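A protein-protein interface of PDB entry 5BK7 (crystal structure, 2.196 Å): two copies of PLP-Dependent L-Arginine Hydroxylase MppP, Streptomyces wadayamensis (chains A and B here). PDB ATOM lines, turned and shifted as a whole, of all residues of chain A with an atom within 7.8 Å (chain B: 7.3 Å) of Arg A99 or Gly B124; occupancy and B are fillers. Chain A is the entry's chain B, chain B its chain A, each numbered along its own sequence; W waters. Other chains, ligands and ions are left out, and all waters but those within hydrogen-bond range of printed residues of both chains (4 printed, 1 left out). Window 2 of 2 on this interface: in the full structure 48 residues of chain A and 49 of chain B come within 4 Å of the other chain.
The side-chain amide nitrogen (ND2) of Asn B125 sits close to the guanidinium group (NE) of Arg A99 (3.5 Å).
The guanidinium group (NH2) of Arg B99 is in salt-bridge range of the side-chain carboxylate (OE1) of Glu A95.
O of Gly A124 lies within hydrogen-bond range of NH1 of Arg B99, 3.4 Å away.
The side-chain carboxylate of Glu B95 lies within salt-bridge range of the guanidinium group of Arg A99 (2.7 Å).
OE1 of Glu B95 sits close to OE2 of Glu A95 (2.3 Å).
NZ of Lys A245 is in salt-bridge range of OD2 of Asp A249 (3.9 Å).
O of Leu B121 lies within hydrogen-bond range of ND2 of Asn B125 (2.9 Å).
ND2 of Asn A125 is in hydrogen-bond range of O of Leu A121, 3.1 Å away.
OD1 of Asp B120 lies within salt-bridge range of NH1 of Arg B123 (3.8 Å).
OE1 of Glu A95 lies within hydrogen-bond range of ND2 of Asn A125, 3.2 Å away.
ND2 of Asn B125 lies within hydrogen-bond range of OE2 of Glu B95, at 3.2 Å.
Among the printed residues, merely in contact across the chains: Arg A99 with Leu B121 (3.6 Å), Arg A99 with Gly B124 (3.6 Å), Leu A121 with Arg B99 (3.6 Å), Asn A125 with Arg B99 (3.6 Å), Asp A249 with Asp B120 (3.6 Å) and Asp A249 with Leu B121 (3.5 Å).
Printed residues of chain B within 4 Å of Arg A99: Glu B95 (2.7 Å), Leu B121 (3.6 Å), Gly B124 (3.6 Å) and Asn B125 (3.5 Å).
Of the printed residues of chain A, Gly B124 touches Arg A99.
No residue of chain B comes within 4 Å of Ala A98.
Printed residues of chain B within 4 Å of Leu A121: Arg B99 (3.6 Å).
Of the printed residues of chain B, Asp A249 touches Asp B120 (3.6 Å) and Leu B121 (3.5 Å).
Ile A96 touches none of the printed residues of chain B.
The nearest printed residue of chain A that does not touch Leu B121 is Ile A250 (4.1 Å).
Of the 26 printed residues of chain A, 6 touch a printed residue of chain B.
Printed residues of chain A that touch a printed residue of chain B: Glu A95, Arg A99, Leu A121, Gly A124, Asn A125 and Asp A249.
Hydrophobic or aromatic side chains of chain A within 4 Å of the printed part of chain B: Leu A121.
Along chain A the printed residues that touch a printed residue of chain B span positions 95 to 249.
Of the 13 printed residues of chain B, 6 touch a printed residue of chain A.
Printed residues of chain B that touch a printed residue of chain A: Glu B95, Arg B99, Asp B120, Leu B121, Gly B124 and Asn B125.
Among the printed residues, 11 pairs touch across the chains.
Among the printed residues, Asp or Glu carboxylates within 4 Å of a Lys or Arg side-chain nitrogen of the other chain: Glu A95 with Arg B99 and Arg A99 with Glu B95.
Glu A95 touches Arg B99, and with the chains exchanged Arg A99 touches Glu B95.
Arg A99 touches Leu B121, and with the chains exchanged Leu A121 touches Arg B99.
Arg A99 touches Gly B124, and with the chains exchanged Gly A124 touches Arg B99.
Arg A99 touches Asn B125, and with the chains exchanged Asn A125 touches Arg B99.
Water W3 lies within hydrogen-bond range of OD1 of Asp A249 (2.5 Å) and OD2 of Asp B120 (2.6 Å).
Water W1 lies within hydrogen-bond range of the guanidinium group (NH1) of Arg B99 (2.5 Å) and the backbone carbonyl oxygen (O) of Gly A124 (2.7 Å).
Water W4 bridges O of Gly B124 and NH1 of Arg A99.
Water W2 lies within hydrogen-bond range of the side-chain carboxylate (OD2) of Asp A249 (2.8 Å), the guanidinium group (NH1) of Arg A99 (2.8 Å) and the backbone carbonyl oxygen (O) of Asp B120 (3.1 Å).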
ATOM      1  N   SER A  93     -10.541 -14.389 -12.593  1.00  0.00           N
ATOM      2  CA  SER A  93     -10.288 -13.712 -11.320  1.00  0.00           C
ATOM      3  C   SER A  93      -8.874 -13.160 -11.292  1.00  0.00           C
ATOM      4  O   SER A  93      -8.625 -12.072 -10.775  1.00  0.00           O
ATOM      5  CB  SER A  93     -10.424 -14.673 -10.130  1.00  0.00           C
ATOM      6  OG  SER A  93     -11.669 -15.331 -10.096  1.00  0.00           O
ATOM      7  N   MET A  94      -7.929 -13.927 -11.792  1.00  0.00           N
ATOM      8  CA  MET A  94      -6.565 -13.460 -11.787  1.00  0.00           C
ATOM      9  C   MET A  94      -6.404 -12.211 -12.676  1.00  0.00           C
ATOM     10  O   MET A  94      -5.828 -11.197 -12.250  1.00  0.00           O
ATOM     11  CB  MET A  94      -5.678 -14.612 -12.220  1.00  0.00           C
ATOM     12  CG  MET A  94      -4.160 -14.367 -12.039  1.00  0.00           C
ATOM     13  SD  MET A  94      -3.687 -13.957 -10.349  1.00  0.00           S
ATOM     14  CE  MET A  94      -2.321 -12.830 -10.682  1.00  0.00           C
ATOM     15  N   GLU A  95      -6.928 -12.243 -13.909  1.00  0.00           N
ATOM     16  CA  GLU A  95      -6.820 -11.047 -14.744  1.00  0.00           C
ATOM     17  C   GLU A  95      -7.435  -9.827 -14.048  1.00  0.00           C
ATOM     18  O   GLU A  95      -6.898  -8.728 -14.115  1.00  0.00           O
ATOM     19  CB  GLU A  95      -7.492 -11.297 -16.102  1.00  0.00           C
ATOM     20  CG  GLU A  95      -7.641 -10.077 -17.005  1.00  0.00           C
ATOM     21  CD  GLU A  95      -6.428  -9.807 -17.858  1.00  0.00           C
ATOM     22  OE1 GLU A  95      -5.418 -10.507 -17.684  1.00  0.00           O
ATOM     23  OE2 GLU A  95      -6.479  -8.893 -18.708  1.00  0.00           O
ATOM     24  N   ILE A  96      -8.586  -9.977 -13.415  1.00  0.00           N
ATOM     25  CA  ILE A  96      -9.210  -8.820 -12.759  1.00  0.00           C
ATOM     26  C   ILE A  96      -8.253  -8.221 -11.737  1.00  0.00           C
ATOM     27  O   ILE A  96      -8.090  -6.997 -11.640  1.00  0.00           O
ATOM     28  CB  ILE A  96     -10.532  -9.235 -12.092  1.00  0.00           C
ATOM     29  CG1 ILE A  96     -11.625  -9.468 -13.166  1.00  0.00           C
ATOM     30  CG2 ILE A  96     -10.983  -8.210 -11.072  1.00  0.00           C
ATOM     31  CD1 ILE A  96     -12.870 -10.148 -12.635  1.00  0.00           C
ATOM     32  N   LEU A  97      -7.627  -9.092 -10.941  1.00  0.00           N
ATOM     33  CA  LEU A  97      -6.723  -8.667  -9.880  1.00  0.00           C
ATOM     34  C   LEU A  97      -5.466  -8.059 -10.465  1.00  0.00           C
ATOM     35  O   LEU A  97      -4.986  -7.009 -10.005  1.00  0.00           O
ATOM     36  CB  LEU A  97      -6.379  -9.874  -8.998  1.00  0.00           C
ATOM     37  CG  LEU A  97      -5.239  -9.686  -7.964  1.00  0.00           C
ATOM     38  CD1 LEU A  97      -5.675  -8.711  -6.894  1.00  0.00           C
ATOM     39  CD2 LEU A  97      -4.803 -10.973  -7.333  1.00  0.00           C
ATOM     40  N   ALA A  98      -4.890  -8.715 -11.468  1.00  0.00           N
ATOM     41  CA  ALA A  98      -3.664  -8.176 -12.042  1.00  0.00           C
ATOM     42  C   ALA A  98      -3.916  -6.799 -12.629  1.00  0.00           C
ATOM     43  O   ALA A  98      -3.192  -5.855 -12.342  1.00  0.00           O
ATOM     44  CB  ALA A  98      -3.113  -9.113 -13.097  1.00  0.00           C
ATOM     45  N   ARG A  99      -4.971  -6.655 -13.422  1.00  0.00           N
ATOM     46  CA  ARG A  99      -5.277  -5.345 -13.973  1.00  0.00           C
ATOM     47  C   ARG A  99      -5.585  -4.349 -12.858  1.00  0.00           C
ATOM     48  O   ARG A  99      -5.247  -3.162 -12.964  1.00  0.00           O
ATOM     49  CB  ARG A  99      -6.433  -5.462 -14.978  1.00  0.00           C
ATOM     50  CG  ARG A  99      -6.804  -4.168 -15.662  1.00  0.00           C
ATOM     51  CD  ARG A  99      -6.761  -4.252 -17.140  1.00  0.00           C
ATOM     52  NE  ARG A  99      -8.024  -4.700 -17.716  1.00  0.00           N
ATOM     53  CZ  ARG A  99      -9.187  -4.083 -17.584  1.00  0.00           C
ATOM     54  NH1 ARG A  99      -9.315  -2.962 -16.879  1.00  0.00           N
ATOM     55  NH2 ARG A  99     -10.253  -4.594 -18.178  1.00  0.00           N
ATOM     56  N   SER A 100      -6.193  -4.822 -11.766  1.00  0.00           N
ATOM     57  CA  SER A 100      -6.545  -3.938 -10.670  1.00  0.00           C
ATOM     58  C   SER A 100      -5.293  -3.402  -9.982  1.00  0.00           C
ATOM     59  O   SER A 100      -5.180  -2.197  -9.729  1.00  0.00           O
ATOM     60  CB  SER A 100      -7.436  -4.684  -9.670  1.00  0.00           C
ATOM     61  OG  SER A 100      -8.777  -4.751 -10.165  1.00  0.00           O
ATOM     62  N   LEU A 101      -4.361  -4.299  -9.655  1.00  0.00           N
ATOM     63  CA  LEU A 101      -3.068  -3.915  -9.103  1.00  0.00           C
ATOM     64  C   LEU A 101      -2.406  -2.838  -9.932  1.00  0.00           C
ATOM     65  O   LEU A 101      -1.901  -1.849  -9.389  1.00  0.00           O
ATOM     66  CB  LEU A 101      -2.151  -5.125  -9.057  1.00  0.00           C
ATOM     67  CG  LEU A 101      -2.461  -6.146  -7.970  1.00  0.00           C
ATOM     68  CD1 LEU A 101      -1.761  -7.478  -8.327  1.00  0.00           C
ATOM     69  CD2 LEU A 101      -2.090  -5.624  -6.595  1.00  0.00           C
ATOM     70  N   SER A 102      -2.365  -3.036 -11.259  1.00  0.00           N
ATOM     71  CA  SER A 102      -1.502  -2.227 -12.118  1.00  0.00           C
ATOM     72  C   SER A 102      -1.734  -0.743 -11.902  1.00  0.00           C
ATOM     73  O   SER A 102      -0.819   0.058 -12.094  1.00  0.00           O
ATOM     74  CB  SER A 102      -1.717  -2.577 -13.594  1.00  0.00           C
ATOM     75  OG  SER A 102      -2.992  -2.159 -14.042  1.00  0.00           O
ATOM     76  N   ALA A 103      -2.925  -0.365 -11.448  1.00  0.00           N
ATOM     77  CA  ALA A 103      -3.219   1.041 -11.209  1.00  0.00           C
ATOM     78  C   ALA A 103      -2.379   1.657 -10.079  1.00  0.00           C
ATOM     79  O   ALA A 103      -2.163   2.875 -10.072  1.00  0.00           O
ATOM     80  CB  ALA A 103      -4.706   1.190 -10.913  1.00  0.00           C
ATOM     81  N   SER A 104      -1.899   0.862  -9.116  1.00  0.00           N
ATOM     82  CA  SER A 104      -1.341   1.442  -7.898  1.00  0.00           C
ATOM     83  C   SER A 104      -0.108   0.699  -7.395  1.00  0.00           C
ATOM     84  O   SER A 104       0.420   1.038  -6.318  1.00  0.00           O
ATOM     85  CB  SER A 104      -2.388   1.449  -6.797  1.00  0.00           C
ATOM     86  OG  SER A 104      -2.420   0.162  -6.216  1.00  0.00           O
ATOM     87  N   LEU A 121       0.157 -13.392 -16.654  1.00  0.00           N
ATOM     88  CA  LEU A 121      -0.893 -12.392 -16.454  1.00  0.00           C
ATOM     89  C   LEU A 121      -0.373 -11.172 -15.705  1.00  0.00           C
ATOM     90  O   LEU A 121      -0.715 -10.040 -16.049  1.00  0.00           O
ATOM     91  CB  LEU A 121      -2.097 -12.998 -15.709  1.00  0.00           C
ATOM     92  CG  LEU A 121      -2.943 -13.955 -16.548  1.00  0.00           C
ATOM     93  CD1 LEU A 121      -3.842 -14.847 -15.692  1.00  0.00           C
ATOM     94  CD2 LEU A 121      -3.786 -13.169 -17.573  1.00  0.00           C
ATOM     95  N   LEU A 122       0.412 -11.364 -14.650  1.00  0.00           N
ATOM     96  CA  LEU A 122       0.889 -10.201 -13.910  1.00  0.00           C
ATOM     97  C   LEU A 122       1.769  -9.328 -14.795  1.00  0.00           C
ATOM     98  O   LEU A 122       1.631  -8.094 -14.815  1.00  0.00           O
ATOM     99  CB  LEU A 122       1.644 -10.639 -12.657  1.00  0.00           C
ATOM    100  CG  LEU A 122       0.737 -11.021 -11.474  1.00  0.00           C
ATOM    101  CD1 LEU A 122       1.565 -11.726 -10.419  1.00  0.00           C
ATOM    102  CD2 LEU A 122      -0.023  -9.803 -10.878  1.00  0.00           C
ATOM    103  N   GLY A 124       1.730  -9.285 -18.125  1.00  0.00           N
ATOM    104  CA  GLY A 124       1.007  -8.754 -19.259  1.00  0.00           C
ATOM    105  C   GLY A 124       0.239  -7.513 -18.906  1.00  0.00           C
ATOM    106  O   GLY A 124      -0.086  -6.721 -19.797  1.00  0.00           O
ATOM    107  N   ASN A 125      -0.078  -7.348 -17.621  1.00  0.00           N
ATOM    108  CA  ASN A 125      -0.756  -6.178 -17.073  1.00  0.00           C
ATOM    109  C   ASN A 125       0.228  -5.139 -16.508  1.00  0.00           C
ATOM    110  O   ASN A 125      -0.176  -4.156 -15.869  1.00  0.00           O
ATOM    111  CB  ASN A 125      -1.758  -6.641 -16.014  1.00  0.00           C
ATOM    112  CG  ASN A 125      -3.072  -7.128 -16.627  1.00  0.00           C
ATOM    113  OD1 ASN A 125      -3.958  -6.326 -16.939  1.00  0.00           O
ATOM    114  ND2 ASN A 125      -3.202  -8.434 -16.794  1.00  0.00           N
ATOM    115  N   GLY A 126       1.508  -5.327 -16.753  1.00  0.00           N
ATOM    116  CA  GLY A 126       2.457  -4.262 -16.534  1.00  0.00           C
ATOM    117  C   GLY A 126       3.200  -4.312 -15.227  1.00  0.00           C
ATOM    118  O   GLY A 126       3.875  -3.331 -14.885  1.00  0.00           O
ATOM    119  N   LEU A 127       3.116  -5.420 -14.499  1.00  0.00           N
ATOM    120  CA  LEU A 127       3.794  -5.550 -13.225  1.00  0.00           C
ATOM    121  C   LEU A 127       5.141  -6.236 -13.408  1.00  0.00           C
ATOM    122  O   LEU A 127       5.288  -7.135 -14.241  1.00  0.00           O
ATOM    123  CB  LEU A 127       2.910  -6.321 -12.262  1.00  0.00           C
ATOM    124  CG  LEU A 127       1.741  -5.417 -11.911  1.00  0.00           C
ATOM    125  CD1 LEU A 127       0.482  -6.206 -11.761  1.00  0.00           C
ATOM    126  CD2 LEU A 127       2.047  -4.635 -10.642  1.00  0.00           C
ATOM    127  N   LEU A 241      -8.076  -1.565  -4.220  1.00  0.00           N
ATOM    128  CA  LEU A 241      -7.862  -1.888  -5.615  1.00  0.00           C
ATOM    129  C   LEU A 241      -9.210  -1.859  -6.306  1.00  0.00           C
ATOM    130  O   LEU A 241     -10.228  -2.119  -5.659  1.00  0.00           O
ATOM    131  CB  LEU A 241      -7.249  -3.273  -5.783  1.00  0.00           C
ATOM    132  CG  LEU A 241      -5.748  -3.478  -5.677  1.00  0.00           C
ATOM    133  CD1 LEU A 241      -5.184  -2.442  -4.747  1.00  0.00           C
ATOM    134  CD2 LEU A 241      -5.480  -4.882  -5.247  1.00  0.00           C
ATOM    135  N   PRO A 242      -9.271  -1.500  -7.593  1.00  0.00           N
ATOM    136  CA  PRO A 242     -10.573  -1.426  -8.298  1.00  0.00           C
ATOM    137  C   PRO A 242     -11.111  -2.790  -8.765  1.00  0.00           C
ATOM    138  O   PRO A 242     -11.655  -2.887  -9.872  1.00  0.00           O
ATOM    139  CB  PRO A 242     -10.258  -0.504  -9.487  1.00  0.00           C
ATOM    140  CG  PRO A 242      -8.769  -0.753  -9.777  1.00  0.00           C
ATOM    141  CD  PRO A 242      -8.151  -1.001  -8.411  1.00  0.00           C
ATOM    142  N   VAL A 243     -10.961  -3.860  -7.956  1.00  0.00           N
ATOM    143  CA  VAL A 243     -11.443  -5.181  -8.379  1.00  0.00           C
ATOM    144  C   VAL A 243     -12.961  -5.201  -8.612  1.00  0.00           C
ATOM    145  O   VAL A 243     -13.437  -5.944  -9.475  1.00  0.00           O
ATOM    146  CB  VAL A 243     -11.026  -6.289  -7.384  1.00  0.00           C
ATOM    147  CG1 VAL A 243      -9.547  -6.478  -7.408  1.00  0.00           C
ATOM    148  CG2 VAL A 243     -11.506  -6.010  -5.981  1.00  0.00           C
ATOM    149  N   LYS A 245     -15.024  -2.705  -9.754  1.00  0.00           N
ATOM    150  CA  LYS A 245     -15.349  -2.061 -11.021  1.00  0.00           C
ATOM    151  C   LYS A 245     -14.864  -2.891 -12.208  1.00  0.00           C
ATOM    152  O   LYS A 245     -15.592  -3.085 -13.186  1.00  0.00           O
ATOM    153  CB  LYS A 245     -14.733  -0.667 -11.049  1.00  0.00           C
ATOM    154  CG  LYS A 245     -15.065   0.087 -12.313  1.00  0.00           C
ATOM    155  CD  LYS A 245     -14.290   1.395 -12.404  1.00  0.00           C
ATOM    156  CE  LYS A 245     -14.881   2.336 -13.442  1.00  0.00           C
ATOM    157  NZ  LYS A 245     -14.613   1.868 -14.806  1.00  0.00           N
ATOM    158  N   ILE A 246     -13.631  -3.381 -12.155  1.00  0.00           N
ATOM    159  CA  ILE A 246     -13.128  -4.200 -13.252  1.00  0.00           C
ATOM    160  C   ILE A 246     -13.940  -5.499 -13.374  1.00  0.00           C
ATOM    161  O   ILE A 246     -14.316  -5.921 -14.475  1.00  0.00           O
ATOM    162  CB  ILE A 246     -11.622  -4.445 -13.044  1.00  0.00           C
ATOM    163  CG1 ILE A 246     -10.863  -3.118 -13.242  1.00  0.00           C
ATOM    164  CG2 ILE A 246     -11.088  -5.469 -14.020  1.00  0.00           C
ATOM    165  CD1 ILE A 246      -9.346  -3.200 -13.195  1.00  0.00           C
ATOM    166  N   TYR A 247     -14.292  -6.117 -12.250  1.00  0.00           N
ATOM    167  CA  TYR A 247     -15.216  -7.243 -12.314  1.00  0.00           C
ATOM    168  C   TYR A 247     -16.477  -6.904 -13.105  1.00  0.00           C
ATOM    169  O   TYR A 247     -16.923  -7.707 -13.932  1.00  0.00           O
ATOM    170  CB  TYR A 247     -15.616  -7.699 -10.905  1.00  0.00           C
ATOM    171  CG  TYR A 247     -16.636  -8.826 -10.899  1.00  0.00           C
ATOM    172  CD1 TYR A 247     -16.244 -10.156 -10.912  1.00  0.00           C
ATOM    173  CD2 TYR A 247     -17.986  -8.554 -10.937  1.00  0.00           C
ATOM    174  CE1 TYR A 247     -17.191 -11.182 -10.913  1.00  0.00           C
ATOM    175  CE2 TYR A 247     -18.927  -9.570 -10.944  1.00  0.00           C
ATOM    176  CZ  TYR A 247     -18.525 -10.880 -10.912  1.00  0.00           C
ATOM    177  OH  TYR A 247     -19.501 -11.877 -10.897  1.00  0.00           O
ATOM    178  N   ASP A 249     -16.936  -4.589 -15.301  1.00  0.00           N
ATOM    179  CA  ASP A 249     -16.657  -4.399 -16.724  1.00  0.00           C
ATOM    180  C   ASP A 249     -16.687  -5.721 -17.467  1.00  0.00           C
ATOM    181  O   ASP A 249     -17.163  -5.786 -18.609  1.00  0.00           O
ATOM    182  CB  ASP A 249     -15.302  -3.722 -16.918  1.00  0.00           C
ATOM    183  CG  ASP A 249     -15.331  -2.296 -16.505  1.00  0.00           C
ATOM    184  OD1 ASP A 249     -16.455  -1.704 -16.506  1.00  0.00           O
ATOM    185  OD2 ASP A 249     -14.231  -1.814 -16.170  1.00  0.00           O
ATOM    186  N   ILE A 250     -16.226  -6.792 -16.827  1.00  0.00           N
ATOM    187  CA  ILE A 250     -16.134  -8.100 -17.491  1.00  0.00           C
ATOM    188  C   ILE A 250     -17.431  -8.919 -17.434  1.00  0.00           C
ATOM    189  O   ILE A 250     -17.818  -9.507 -18.446  1.00  0.00           O
ATOM    190  CB  ILE A 250     -14.960  -8.862 -16.893  1.00  0.00           C
ATOM    191  CG1 ILE A 250     -13.687  -8.110 -17.302  1.00  0.00           C
ATOM    192  CG2 ILE A 250     -14.979 -10.310 -17.391  1.00  0.00           C
ATOM    193  CD1 ILE A 250     -12.525  -8.581 -16.654  1.00  0.00           C
ATOM    194  N   GLU B  95     -11.761  -8.473 -23.493  1.00  0.00           N
ATOM    195  CA  GLU B  95     -10.584  -8.213 -22.662  1.00  0.00           C
ATOM    196  C   GLU B  95      -9.329  -8.672 -23.371  1.00  0.00           C
ATOM    197  O   GLU B  95      -8.320  -7.959 -23.392  1.00  0.00           O
ATOM    198  CB  GLU B  95     -10.709  -8.901 -21.296  1.00  0.00           C
ATOM    199  CG  GLU B  95      -9.419  -8.847 -20.426  1.00  0.00           C
ATOM    200  CD  GLU B  95      -9.158  -7.475 -19.795  1.00  0.00           C
ATOM    201  OE1 GLU B  95      -8.165  -7.342 -19.037  1.00  0.00           O
ATOM    202  OE2 GLU B  95      -9.941  -6.550 -20.051  1.00  0.00           O
ATOM    203  N   ALA B  98      -8.765  -6.070 -26.251  1.00  0.00           N
ATOM    204  CA  ALA B  98      -8.337  -4.768 -25.777  1.00  0.00           C
ATOM    205  C   ALA B  98      -6.898  -4.842 -25.260  1.00  0.00           C
ATOM    206  O   ALA B  98      -6.062  -3.999 -25.599  1.00  0.00           O
ATOM    207  CB  ALA B  98      -9.308  -4.280 -24.711  1.00  0.00           C
ATOM    208  N   ARG B  99      -6.555  -5.885 -24.498  1.00  0.00           N
ATOM    209  CA  ARG B  99      -5.203  -5.905 -23.999  1.00  0.00           C
ATOM    210  C   ARG B  99      -4.205  -6.196 -25.126  1.00  0.00           C
ATOM    211  O   ARG B  99      -3.068  -5.709 -25.085  1.00  0.00           O
ATOM    212  CB  ARG B  99      -5.081  -6.904 -22.861  1.00  0.00           C
ATOM    213  CG  ARG B  99      -3.654  -6.875 -22.290  1.00  0.00           C
ATOM    214  CD  ARG B  99      -3.654  -6.873 -20.834  1.00  0.00           C
ATOM    215  NE  ARG B  99      -4.051  -8.171 -20.305  1.00  0.00           N
ATOM    216  CZ  ARG B  99      -3.304  -9.262 -20.372  1.00  0.00           C
ATOM    217  NH1 ARG B  99      -2.105  -9.233 -20.960  1.00  0.00           N
ATOM    218  NH2 ARG B  99      -3.753 -10.386 -19.819  1.00  0.00           N
ATOM    219  N   ILE B 118     -17.616  -2.063 -23.717  1.00  0.00           N
ATOM    220  CA  ILE B 118     -16.611  -2.078 -24.792  1.00  0.00           C
ATOM    221  C   ILE B 118     -15.638  -0.919 -24.604  1.00  0.00           C
ATOM    222  O   ILE B 118     -14.418  -1.069 -24.733  1.00  0.00           O
ATOM    223  CB  ILE B 118     -17.284  -2.023 -26.186  1.00  0.00           C
ATOM    224  CG1 ILE B 118     -18.200  -3.222 -26.400  1.00  0.00           C
ATOM    225  CG2 ILE B 118     -16.246  -1.947 -27.322  1.00  0.00           C
ATOM    226  CD1 ILE B 118     -19.064  -3.088 -27.602  1.00  0.00           C
ATOM    227  N   ALA B 119     -16.181   0.274 -24.359  1.00  0.00           N
ATOM    228  CA  ALA B 119     -15.337   1.435 -24.104  1.00  0.00           C
ATOM    229  C   ALA B 119     -14.573   1.284 -22.789  1.00  0.00           C
ATOM    230  O   ALA B 119     -13.372   1.595 -22.716  1.00  0.00           O
ATOM    231  CB  ALA B 119     -16.220   2.691 -24.119  1.00  0.00           C
ATOM    232  N   ASP B 120     -15.253   0.799 -21.733  1.00  0.00           N
ATOM    233  CA  ASP B 120     -14.578   0.584 -20.457  1.00  0.00           C
ATOM    234  C   ASP B 120     -13.442  -0.414 -20.594  1.00  0.00           C
ATOM    235  O   ASP B 120     -12.340  -0.209 -20.051  1.00  0.00           O
ATOM    236  CB  ASP B 120     -15.608   0.158 -19.419  1.00  0.00           C
ATOM    237  CG  ASP B 120     -16.566   1.256 -19.145  1.00  0.00           C
ATOM    238  OD1 ASP B 120     -16.282   2.334 -19.671  1.00  0.00           O
ATOM    239  OD2 ASP B 120     -17.595   1.120 -18.457  1.00  0.00           O
ATOM    240  N   LEU B 121     -13.636  -1.483 -21.347  1.00  0.00           N
ATOM    241  CA  LEU B 121     -12.528  -2.429 -21.380  1.00  0.00           C
ATOM    242  C   LEU B 121     -11.374  -1.840 -22.162  1.00  0.00           C
ATOM    243  O   LEU B 121     -10.209  -2.052 -21.794  1.00  0.00           O
ATOM    244  CB  LEU B 121     -12.952  -3.780 -21.944  1.00  0.00           C
ATOM    245  CG  LEU B 121     -14.006  -4.551 -21.121  1.00  0.00           C
ATOM    246  CD1 LEU B 121     -14.343  -5.821 -21.845  1.00  0.00           C
ATOM    247  CD2 LEU B 121     -13.511  -4.807 -19.705  1.00  0.00           C
ATOM    248  N   LEU B 122     -11.678  -1.065 -23.226  1.00  0.00           N
ATOM    249  CA  LEU B 122     -10.599  -0.424 -23.983  1.00  0.00           C
ATOM    250  C   LEU B 122      -9.873   0.633 -23.146  1.00  0.00           C
ATOM    251  O   LEU B 122      -8.645   0.585 -23.000  1.00  0.00           O
ATOM    252  CB  LEU B 122     -11.148   0.193 -25.273  1.00  0.00           C
ATOM    253  CG  LEU B 122     -11.650  -0.839 -26.274  1.00  0.00           C
ATOM    254  CD1 LEU B 122     -12.486  -0.146 -27.337  1.00  0.00           C
ATOM    255  CD2 LEU B 122     -10.477  -1.584 -26.862  1.00  0.00           C
ATOM    256  N   ARG B 123     -10.608   1.602 -22.597  1.00  0.00           N
ATOM    257  CA  ARG B 123      -9.951   2.605 -21.772  1.00  0.00           C
ATOM    258  C   ARG B 123      -9.224   1.953 -20.609  1.00  0.00           C
ATOM    259  O   ARG B 123      -8.065   2.279 -20.336  1.00  0.00           O
ATOM    260  CB  ARG B 123     -10.967   3.625 -21.259  1.00  0.00           C
ATOM    261  CG  ARG B 123     -11.560   4.555 -22.278  1.00  0.00           C
ATOM    262  CD  ARG B 123     -11.951   5.812 -21.531  1.00  0.00           C
ATOM    263  NE  ARG B 123     -12.994   6.631 -22.139  1.00  0.00           N
ATOM    264  CZ  ARG B 123     -14.307   6.451 -21.966  1.00  0.00           C
ATOM    265  NH1 ARG B 123     -14.775   5.444 -21.237  1.00  0.00           N
ATOM    266  NH2 ARG B 123     -15.170   7.280 -22.545  1.00  0.00           N
ATOM    267  N   GLY B 124      -9.850   0.954 -19.973  1.00  0.00           N
ATOM    268  CA  GLY B 124      -9.186   0.211 -18.902  1.00  0.00           C
ATOM    269  C   GLY B 124      -7.850  -0.398 -19.291  1.00  0.00           C
ATOM    270  O   GLY B 124      -6.999  -0.658 -18.428  1.00  0.00           O
ATOM    271  N   ASN B 125      -7.646  -0.686 -20.567  1.00  0.00           N
ATOM    272  CA  ASN B 125      -6.398  -1.306 -20.979  1.00  0.00           C
ATOM    273  C   ASN B 125      -5.438  -0.304 -21.580  1.00  0.00           C
ATOM    274  O   ASN B 125      -4.462  -0.702 -22.218  1.00  0.00           O
ATOM    275  CB  ASN B 125      -6.680  -2.424 -21.953  1.00  0.00           C
ATOM    276  CG  ASN B 125      -6.979  -3.718 -21.259  1.00  0.00           C
ATOM    277  OD1 ASN B 125      -6.064  -4.398 -20.831  1.00  0.00           O
ATOM    278  ND2 ASN B 125      -8.264  -4.064 -21.135  1.00  0.00           N
ATOM    279  N   GLY B 126      -5.691   0.981 -21.377  1.00  0.00           N
ATOM    280  CA  GLY B 126      -4.764   2.000 -21.829  1.00  0.00           C
ATOM    281  C   GLY B 126      -5.022   2.653 -23.181  1.00  0.00           C
ATOM    282  O   GLY B 126      -4.163   3.395 -23.644  1.00  0.00           O
ATOM    283  N   LEU B 127      -6.168   2.437 -23.813  1.00  0.00           N
ATOM    284  CA  LEU B 127      -6.433   2.964 -25.151  1.00  0.00           C
ATOM    285  C   LEU B 127      -7.268   4.218 -24.999  1.00  0.00           C
ATOM    286  O   LEU B 127      -8.087   4.303 -24.075  1.00  0.00           O
ATOM    287  CB  LEU B 127      -7.164   1.932 -26.026  1.00  0.00           C
ATOM    288  CG  LEU B 127      -6.298   0.663 -26.150  1.00  0.00           C
ATOM    289  CD1 LEU B 127      -7.073  -0.584 -25.974  1.00  0.00           C
ATOM    290  CD2 LEU B 127      -5.552   0.593 -27.473  1.00  0.00           C
HETATM  291  O   HOH W   1      -0.365  -7.881 -22.243  1.00  0.00           O
HETATM  292  O   HOH W   2     -11.916  -2.213 -17.688  1.00  0.00           O
HETATM  293  O   HOH W   3     -18.390  -1.340 -18.050  1.00  0.00           O
HETATM  294  O   HOH W   4      -7.887  -0.729 -15.804  1.00  0.00           O
